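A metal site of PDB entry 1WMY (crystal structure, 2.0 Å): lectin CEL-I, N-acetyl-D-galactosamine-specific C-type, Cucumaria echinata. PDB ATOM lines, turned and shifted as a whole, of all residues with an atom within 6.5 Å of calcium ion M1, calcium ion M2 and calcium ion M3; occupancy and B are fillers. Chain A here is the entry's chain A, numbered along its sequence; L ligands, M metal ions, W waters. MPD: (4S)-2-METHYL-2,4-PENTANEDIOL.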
ATOM      1  N   ASP A  77       3.729  -7.331  25.049  1.00  0.00           N
ATOM      2  CA  ASP A  77       3.185  -6.009  24.747  1.00  0.00           C
ATOM      3  C   ASP A  77       2.576  -5.916  23.323  1.00  0.00           C
ATOM      4  O   ASP A  77       2.676  -4.866  22.636  1.00  0.00           O
ATOM      5  CB  ASP A  77       4.242  -4.941  24.956  1.00  0.00           C
ATOM      6  CG  ASP A  77       5.269  -4.894  23.840  1.00  0.00           C
ATOM      7  OD1 ASP A  77       5.530  -5.900  23.166  1.00  0.00           O
ATOM      8  OD2 ASP A  77       5.913  -3.853  23.582  1.00  0.00           O
ATOM      9  N   LYS A  78       1.936  -6.984  22.934  1.00  0.00           N
ATOM     10  CA  LYS A  78       1.176  -7.052  21.707  1.00  0.00           C
ATOM     11  C   LYS A  78       0.072  -6.004  21.631  1.00  0.00           C
ATOM     12  O   LYS A  78      -0.132  -5.407  20.552  1.00  0.00           O
ATOM     13  CB  LYS A  78       0.634  -8.506  21.569  1.00  0.00           C
ATOM     14  CG  LYS A  78      -0.082  -8.890  20.315  1.00  0.00           C
ATOM     15  CD  LYS A  78       0.101 -10.431  19.950  1.00  0.00           C
ATOM     16  CE  LYS A  78      -0.447 -11.377  21.086  1.00  0.00           C
ATOM     17  NZ  LYS A  78      -0.453 -12.906  20.806  1.00  0.00           N
ATOM     18  N   ASN A  80      -0.481  -3.193  23.538  1.00  0.00           N
ATOM     19  CA  ASN A  80      -0.022  -1.855  23.782  1.00  0.00           C
ATOM     20  C   ASN A  80       1.510  -1.867  23.794  1.00  0.00           C
ATOM     21  O   ASN A  80       2.128  -2.120  24.802  1.00  0.00           O
ATOM     22  CB  ASN A  80      -0.575  -1.388  25.124  1.00  0.00           C
ATOM     23  CG  ASN A  80      -2.062  -1.081  25.088  1.00  0.00           C
ATOM     24  OD1 ASN A  80      -2.463   0.039  24.773  1.00  0.00           O
ATOM     25  ND2 ASN A  80      -2.874  -2.103  25.303  1.00  0.00           N
ATOM     26  N   GLU A  81       2.116  -1.486  22.679  1.00  0.00           N
ATOM     27  CA  GLU A  81       3.522  -1.539  22.497  1.00  0.00           C
ATOM     28  C   GLU A  81       4.200  -0.727  23.587  1.00  0.00           C
ATOM     29  O   GLU A  81       3.754   0.379  23.817  1.00  0.00           O
ATOM     30  CB  GLU A  81       3.874  -1.009  21.085  1.00  0.00           C
ATOM     31  CG  GLU A  81       5.395  -0.876  20.857  1.00  0.00           C
ATOM     32  CD  GLU A  81       6.130  -2.213  20.991  1.00  0.00           C
ATOM     33  OE1 GLU A  81       7.204  -2.287  21.637  1.00  0.00           O
ATOM     34  OE2 GLU A  81       5.666  -3.219  20.466  1.00  0.00           O
ATOM     35  N   GLY A  82       5.212  -1.277  24.238  1.00  0.00           N
ATOM     36  CA  GLY A  82       5.980  -0.633  25.315  1.00  0.00           C
ATOM     37  C   GLY A  82       5.366  -0.788  26.709  1.00  0.00           C
ATOM     38  O   GLY A  82       5.994  -0.454  27.657  1.00  0.00           O
ATOM     39  N   PHE A  84       4.130  -3.619  28.789  1.00  0.00           N
ATOM     40  CA  PHE A  84       4.083  -5.066  28.977  1.00  0.00           C
ATOM     41  C   PHE A  84       3.093  -5.433  30.089  1.00  0.00           C
ATOM     42  O   PHE A  84       3.005  -4.719  31.126  1.00  0.00           O
ATOM     43  CB  PHE A  84       5.474  -5.554  29.301  1.00  0.00           C
ATOM     44  CG  PHE A  84       6.373  -5.608  28.106  1.00  0.00           C
ATOM     45  CD1 PHE A  84       6.459  -6.757  27.376  1.00  0.00           C
ATOM     46  CD2 PHE A  84       7.098  -4.498  27.722  1.00  0.00           C
ATOM     47  CE1 PHE A  84       7.295  -6.840  26.259  1.00  0.00           C
ATOM     48  CE2 PHE A  84       7.910  -4.537  26.609  1.00  0.00           C
ATOM     49  CZ  PHE A  84       8.023  -5.730  25.885  1.00  0.00           C
ATOM     50  N   GLY A 100      19.514  -2.229  27.934  1.00  0.00           N
ATOM     51  CA  GLY A 100      19.144  -1.975  26.570  1.00  0.00           C
ATOM     52  C   GLY A 100      17.844  -2.635  26.163  1.00  0.00           C
ATOM     53  O   GLY A 100      17.494  -2.679  24.983  1.00  0.00           O
ATOM     54  N   GLN A 101      17.157  -3.196  27.161  1.00  0.00           N
ATOM     55  CA  GLN A 101      15.839  -3.834  26.932  1.00  0.00           C
ATOM     56  C   GLN A 101      14.723  -3.155  27.760  1.00  0.00           C
ATOM     57  O   GLN A 101      14.989  -2.628  28.805  1.00  0.00           O
ATOM     58  CB  GLN A 101      15.942  -5.297  27.281  1.00  0.00           C
ATOM     59  CG  GLN A 101      17.078  -6.082  26.608  1.00  0.00           C
ATOM     60  CD  GLN A 101      17.002  -6.062  25.124  1.00  0.00           C
ATOM     61  OE1 GLN A 101      15.890  -6.015  24.560  1.00  0.00           O
ATOM     62  NE2 GLN A 101      18.187  -6.073  24.447  1.00  0.00           N
ATOM     63  N   PRO A 102      13.461  -3.235  27.329  1.00  0.00           N
ATOM     64  CA  PRO A 102      13.026  -3.882  26.102  1.00  0.00           C
ATOM     65  C   PRO A 102      13.201  -2.923  24.909  1.00  0.00           C
ATOM     66  O   PRO A 102      12.845  -1.745  25.053  1.00  0.00           O
ATOM     67  CB  PRO A 102      11.552  -4.189  26.389  1.00  0.00           C
ATOM     68  CG  PRO A 102      11.069  -3.124  27.308  1.00  0.00           C
ATOM     69  CD  PRO A 102      12.319  -2.694  28.107  1.00  0.00           C
ATOM     70  N   ASP A 103      13.748  -3.388  23.794  1.00  0.00           N
ATOM     71  CA  ASP A 103      14.084  -2.474  22.667  1.00  0.00           C
ATOM     72  C   ASP A 103      13.189  -2.695  21.437  1.00  0.00           C
ATOM     73  O   ASP A 103      13.249  -1.938  20.485  1.00  0.00           O
ATOM     74  CB  ASP A 103      15.525  -2.602  22.284  1.00  0.00           C
ATOM     75  CG  ASP A 103      15.867  -4.042  21.785  1.00  0.00           C
ATOM     76  OD1 ASP A 103      17.008  -4.295  21.344  1.00  0.00           O
ATOM     77  OD2 ASP A 103      15.016  -4.947  21.788  1.00  0.00           O
ATOM     78  N   ASN A 104      12.268  -3.653  21.479  1.00  0.00           N
ATOM     79  CA  ASN A 104      11.323  -3.861  20.352  1.00  0.00           C
ATOM     80  C   ASN A 104      12.089  -3.977  19.027  1.00  0.00           C
ATOM     81  O   ASN A 104      11.765  -3.279  18.013  1.00  0.00           O
ATOM     82  CB  ASN A 104      10.303  -2.701  20.231  1.00  0.00           C
ATOM     83  CG  ASN A 104       9.050  -3.140  19.434  1.00  0.00           C
ATOM     84  OD1 ASN A 104       8.596  -4.243  19.568  1.00  0.00           O
ATOM     85  ND2 ASN A 104       8.539  -2.249  18.558  1.00  0.00           N
ATOM     86  N   TRP A 105      13.182  -4.731  19.072  1.00  0.00           N
ATOM     87  CA  TRP A 105      14.116  -4.781  17.930  1.00  0.00           C
ATOM     88  C   TRP A 105      13.429  -5.090  16.604  1.00  0.00           C
ATOM     89  O   TRP A 105      12.569  -5.971  16.515  1.00  0.00           O
ATOM     90  CB  TRP A 105      15.242  -5.800  18.205  1.00  0.00           C
ATOM     91  CG  TRP A 105      16.189  -5.856  17.133  1.00  0.00           C
ATOM     92  CD1 TRP A 105      17.182  -4.958  16.871  1.00  0.00           C
ATOM     93  CD2 TRP A 105      16.208  -6.787  16.060  1.00  0.00           C
ATOM     94  NE1 TRP A 105      17.856  -5.303  15.742  1.00  0.00           N
ATOM     95  CE2 TRP A 105      17.275  -6.416  15.198  1.00  0.00           C
ATOM     96  CE3 TRP A 105      15.437  -7.902  15.724  1.00  0.00           C
ATOM     97  CZ2 TRP A 105      17.621  -7.152  14.059  1.00  0.00           C
ATOM     98  CZ3 TRP A 105      15.764  -8.613  14.549  1.00  0.00           C
ATOM     99  CH2 TRP A 105      16.837  -8.228  13.736  1.00  0.00           C
ATOM    100  N   ASN A 107      11.213  -3.415  15.198  1.00  0.00           N
ATOM    101  CA  ASN A 107       9.818  -3.130  15.430  1.00  0.00           C
ATOM    102  C   ASN A 107       8.977  -4.412  15.570  1.00  0.00           C
ATOM    103  O   ASN A 107       7.778  -4.434  15.266  1.00  0.00           O
ATOM    104  CB  ASN A 107       9.253  -2.137  14.346  1.00  0.00           C
ATOM    105  CG  ASN A 107       7.959  -1.353  14.861  1.00  0.00           C
ATOM    106  OD1 ASN A 107       7.721  -1.258  16.094  1.00  0.00           O
ATOM    107  ND2 ASN A 107       7.126  -0.840  13.923  1.00  0.00           N
ATOM    108  N   ALA A 108       9.590  -5.495  16.071  1.00  0.00           N
ATOM    109  CA  ALA A 108       8.958  -6.776  16.049  1.00  0.00           C
ATOM    110  C   ALA A 108       9.184  -7.705  17.230  1.00  0.00           C
ATOM    111  O   ALA A 108       9.172  -8.927  17.020  1.00  0.00           O
ATOM    112  CB  ALA A 108       9.360  -7.557  14.746  1.00  0.00           C
ATOM    113  N   GLU A 109       9.396  -7.168  18.421  1.00  0.00           N
ATOM    114  CA  GLU A 109       9.566  -7.974  19.610  1.00  0.00           C
ATOM    115  C   GLU A 109       8.547  -7.658  20.698  1.00  0.00           C
ATOM    116  O   GLU A 109       8.651  -6.636  21.378  1.00  0.00           O
ATOM    117  CB  GLU A 109      11.003  -7.785  20.169  1.00  0.00           C
ATOM    118  CG  GLU A 109      12.093  -8.144  19.139  1.00  0.00           C
ATOM    119  CD  GLU A 109      13.489  -8.219  19.782  1.00  0.00           C
ATOM    120  OE1 GLU A 109      13.808  -7.348  20.635  1.00  0.00           O
ATOM    121  OE2 GLU A 109      14.254  -9.180  19.501  1.00  0.00           O
ATOM    122  N   ASP A 110       7.567  -8.562  20.875  1.00  0.00           N
ATOM    123  CA  ASP A 110       6.523  -8.319  21.838  1.00  0.00           C
ATOM    124  C   ASP A 110       6.490  -9.328  23.011  1.00  0.00           C
ATOM    125  O   ASP A 110       5.521  -9.400  23.724  1.00  0.00           O
ATOM    126  CB  ASP A 110       5.169  -8.216  21.122  1.00  0.00           C
ATOM    127  CG  ASP A 110       5.077  -6.974  20.235  1.00  0.00           C
ATOM    128  OD1 ASP A 110       4.101  -6.872  19.524  1.00  0.00           O
ATOM    129  OD2 ASP A 110       5.916  -6.014  20.274  1.00  0.00           O
ATOM    130  N   TYR A 111       7.535 -10.114  23.161  1.00  0.00           N
ATOM    131  CA  TYR A 111       7.403 -11.306  23.985  1.00  0.00           C
ATOM    132  C   TYR A 111       8.608 -11.440  24.901  1.00  0.00           C
ATOM    133  O   TYR A 111       9.763 -11.482  24.458  1.00  0.00           O
ATOM    134  CB  TYR A 111       7.317 -12.564  23.146  1.00  0.00           C
ATOM    135  CG  TYR A 111       6.215 -12.520  22.117  1.00  0.00           C
ATOM    136  CD1 TYR A 111       6.494 -12.548  20.778  1.00  0.00           C
ATOM    137  CD2 TYR A 111       4.892 -12.490  22.528  1.00  0.00           C
ATOM    138  CE1 TYR A 111       5.476 -12.513  19.853  1.00  0.00           C
ATOM    139  CE2 TYR A 111       3.869 -12.423  21.664  1.00  0.00           C
ATOM    140  CZ  TYR A 111       4.127 -12.466  20.311  1.00  0.00           C
ATOM    141  OH  TYR A 111       3.070 -12.433  19.415  1.00  0.00           O
ATOM    142  N   ARG A 115      17.032 -14.351  29.864  1.00  0.00           N
ATOM    143  CA  ARG A 115      18.295 -14.881  29.366  1.00  0.00           C
ATOM    144  C   ARG A 115      18.865 -15.885  30.387  1.00  0.00           C
ATOM    145  O   ARG A 115      18.513 -15.825  31.577  1.00  0.00           O
ATOM    146  CB  ARG A 115      19.277 -13.733  29.219  1.00  0.00           C
ATOM    147  CG  ARG A 115      18.887 -12.760  28.115  1.00  0.00           C
ATOM    148  CD  ARG A 115      19.979 -11.752  27.990  1.00  0.00           C
ATOM    149  NE  ARG A 115      19.633 -10.745  27.019  1.00  0.00           N
ATOM    150  CZ  ARG A 115      20.279  -9.616  26.849  1.00  0.00           C
ATOM    151  NH1 ARG A 115      21.368  -9.324  27.598  1.00  0.00           N
ATOM    152  NH2 ARG A 115      19.821  -8.777  25.911  1.00  0.00           N
ATOM    153  N   ASN A 123      14.727 -10.121  28.335  1.00  0.00           N
ATOM    154  CA  ASN A 123      14.802  -9.552  27.007  1.00  0.00           C
ATOM    155  C   ASN A 123      13.410  -9.696  26.363  1.00  0.00           C
ATOM    156  O   ASN A 123      12.625 -10.578  26.729  1.00  0.00           O
ATOM    157  CB  ASN A 123      15.804 -10.355  26.212  1.00  0.00           C
ATOM    158  CG  ASN A 123      15.839  -9.941  24.756  1.00  0.00           C
ATOM    159  OD1 ASN A 123      15.910  -8.770  24.462  1.00  0.00           O
ATOM    160  ND2 ASN A 123      15.839 -10.903  23.864  1.00  0.00           N
ATOM    161  N   ASP A 124      13.077  -8.785  25.444  1.00  0.00           N
ATOM    162  CA  ASP A 124      11.931  -8.973  24.580  1.00  0.00           C
ATOM    163  C   ASP A 124      12.422  -9.573  23.268  1.00  0.00           C
ATOM    164  O   ASP A 124      13.449  -9.174  22.732  1.00  0.00           O
ATOM    165  CB  ASP A 124      11.171  -7.695  24.341  1.00  0.00           C
ATOM    166  CG  ASP A 124      12.017  -6.570  23.713  1.00  0.00           C
ATOM    167  OD1 ASP A 124      13.251  -6.642  23.756  1.00  0.00           O
ATOM    168  OD2 ASP A 124      11.454  -5.588  23.184  1.00  0.00           O
ATOM    169  N   ASN A 125      11.626 -10.490  22.724  1.00  0.00           N
ATOM    170  CA  ASN A 125      11.997 -11.159  21.515  1.00  0.00           C
ATOM    171  C   ASN A 125      10.755 -11.353  20.632  1.00  0.00           C
ATOM    172  O   ASN A 125       9.649 -10.943  20.966  1.00  0.00           O
ATOM    173  CB  ASN A 125      12.698 -12.460  21.882  1.00  0.00           C
ATOM    174  CG  ASN A 125      13.739 -12.907  20.856  1.00  0.00           C
ATOM    175  OD1 ASN A 125      13.560 -12.774  19.648  1.00  0.00           O
ATOM    176  ND2 ASN A 125      14.768 -13.549  21.364  1.00  0.00           N
HETATM  177  C1  MPD L   1      17.316  -9.776  19.171  1.00  0.00           C
HETATM  178  C2  MPD L   1      17.393  -9.750  20.673  1.00  0.00           C
HETATM  179  O2  MPD L   1      16.121  -9.296  21.229  1.00  0.00           O
HETATM  180  CM  MPD L   1      17.703 -11.193  21.066  1.00  0.00           C
HETATM  181  C3  MPD L   1      18.472  -8.793  21.160  1.00  0.00           C
HETATM  182  C4  MPD L   1      18.192  -7.356  20.812  1.00  0.00           C
HETATM  183  O4  MPD L   1      17.460  -6.700  21.818  1.00  0.00           O
HETATM  184  C5  MPD L   1      19.453  -6.573  20.585  1.00  0.00           C
HETATM  185 CA    CA M   1       7.205  -4.730  21.694  1.00  0.00          CA
HETATM  186 CA    CA M   2      15.154  -7.332  22.571  1.00  0.00          CA
HETATM  187 CA    CA M   3       4.540  -4.546  18.907  1.00  0.00          CA
HETATM  188  O   HOH W   1       3.018  -5.005  17.104  1.00  0.00           O
HETATM  189  O   HOH W   2       6.496  -4.838  17.681  1.00  0.00           O
HETATM  190  O   HOH W   3       2.710  -3.981  20.112  1.00  0.00           O
HETATM  191  O   HOH W   4       9.227  -4.178  23.047  1.00  0.00           O
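The backbone NH of Trp 105 lies close to the side-chain carboxylate of Asp 103 (3.3 Å). The backbone NH of Asp 110 lies within hydrogen-bond range of the backbone carbonyl oxygen of Asn 125 (3.2 Å). The side-chain carboxylate (OD2) of Asp 124 lies within hydrogen-bond range of the backbone NH (N) of Asn 104, 2.7 Å away. NE2 of Gln 101 lies close to NH2 of Arg 115 (3.5 Å). The backbone NH (N) of Trp 105 sits close to the side-chain carboxylate (OE1) of Glu 109. The side-chain amide nitrogen (ND2) of Asn 104 is in hydrogen-bond range of the side-chain amide oxygen (OD1) of Asn 107. OD2 of Asp 77 lies close to N of Gly 82 (2.7 Å).
Five residues have an atom within 4 Å of calcium ion M2: Gln 101, Asp 103, Glu 109, Asn 123 and Asp 124. The nearest printed residue that does not touch calcium ion M2 is Trp 105 (4.6 Å).
Calcium ion M1 is bound by OD2 of Asp 110 (2.3 Å), O of Glu 109 (2.4 Å), OE1 of Glu 81 (2.4 Å), OD2 of Asp 77 (2.5 Å), OE2 of Glu 81 (2.5 Å), water W4 (2.5 Å), OD1 of Asp 77 (2.5 Å) and OD1 of Asn 104 (2.6 Å).
Calcium ion M2 is bound by the side-chain carboxylate (OD1) of Asp 124 (2.3 Å). Calcium ion M2 is bound by the side-chain carboxylate (OE1) of Glu 109. Calcium ion M2 is bound by the side-chain amide oxygen (OD1) of Asn 123, 2.5 Å away. OE1 of Gln 101 is bound to calcium ion M2 (2.5 Å). O4 of the ligand binds calcium ion M2, at 2.5 Å. OD2 of Asp 103 is bound to calcium ion M2 (2.5 Å). O of Asp 124 is bound to calcium ion M2 (2.5 Å). Calcium ion M2 is bound by O2 of the ligand, 2.6 Å away. Calcium ion M2 has eight donor atoms within binding distance.
Water W3 is bound to calcium ion M3 (2.3 Å). Water W2 is bound to calcium ion M3 (2.3 Å). Calcium ion M3 is bound by OE2 of Glu 81, 2.3 Å away. Water W1 is bound to calcium ion M3 (2.4 Å). OD2 of Asp 110 binds calcium ion M3 (2.4 Å). Calcium ion M3 is bound by OD1 of Asp 110 (2.4 Å). Calcium ion M3 has six donor atoms within binding distance.
Water W4 bridges OD2 of Asp 124 and N of Asn 104. Water W2 lies within hydrogen-bond range of the backbone carbonyl oxygen of Asn 107 and the side-chain amide nitrogen of Asn 104.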
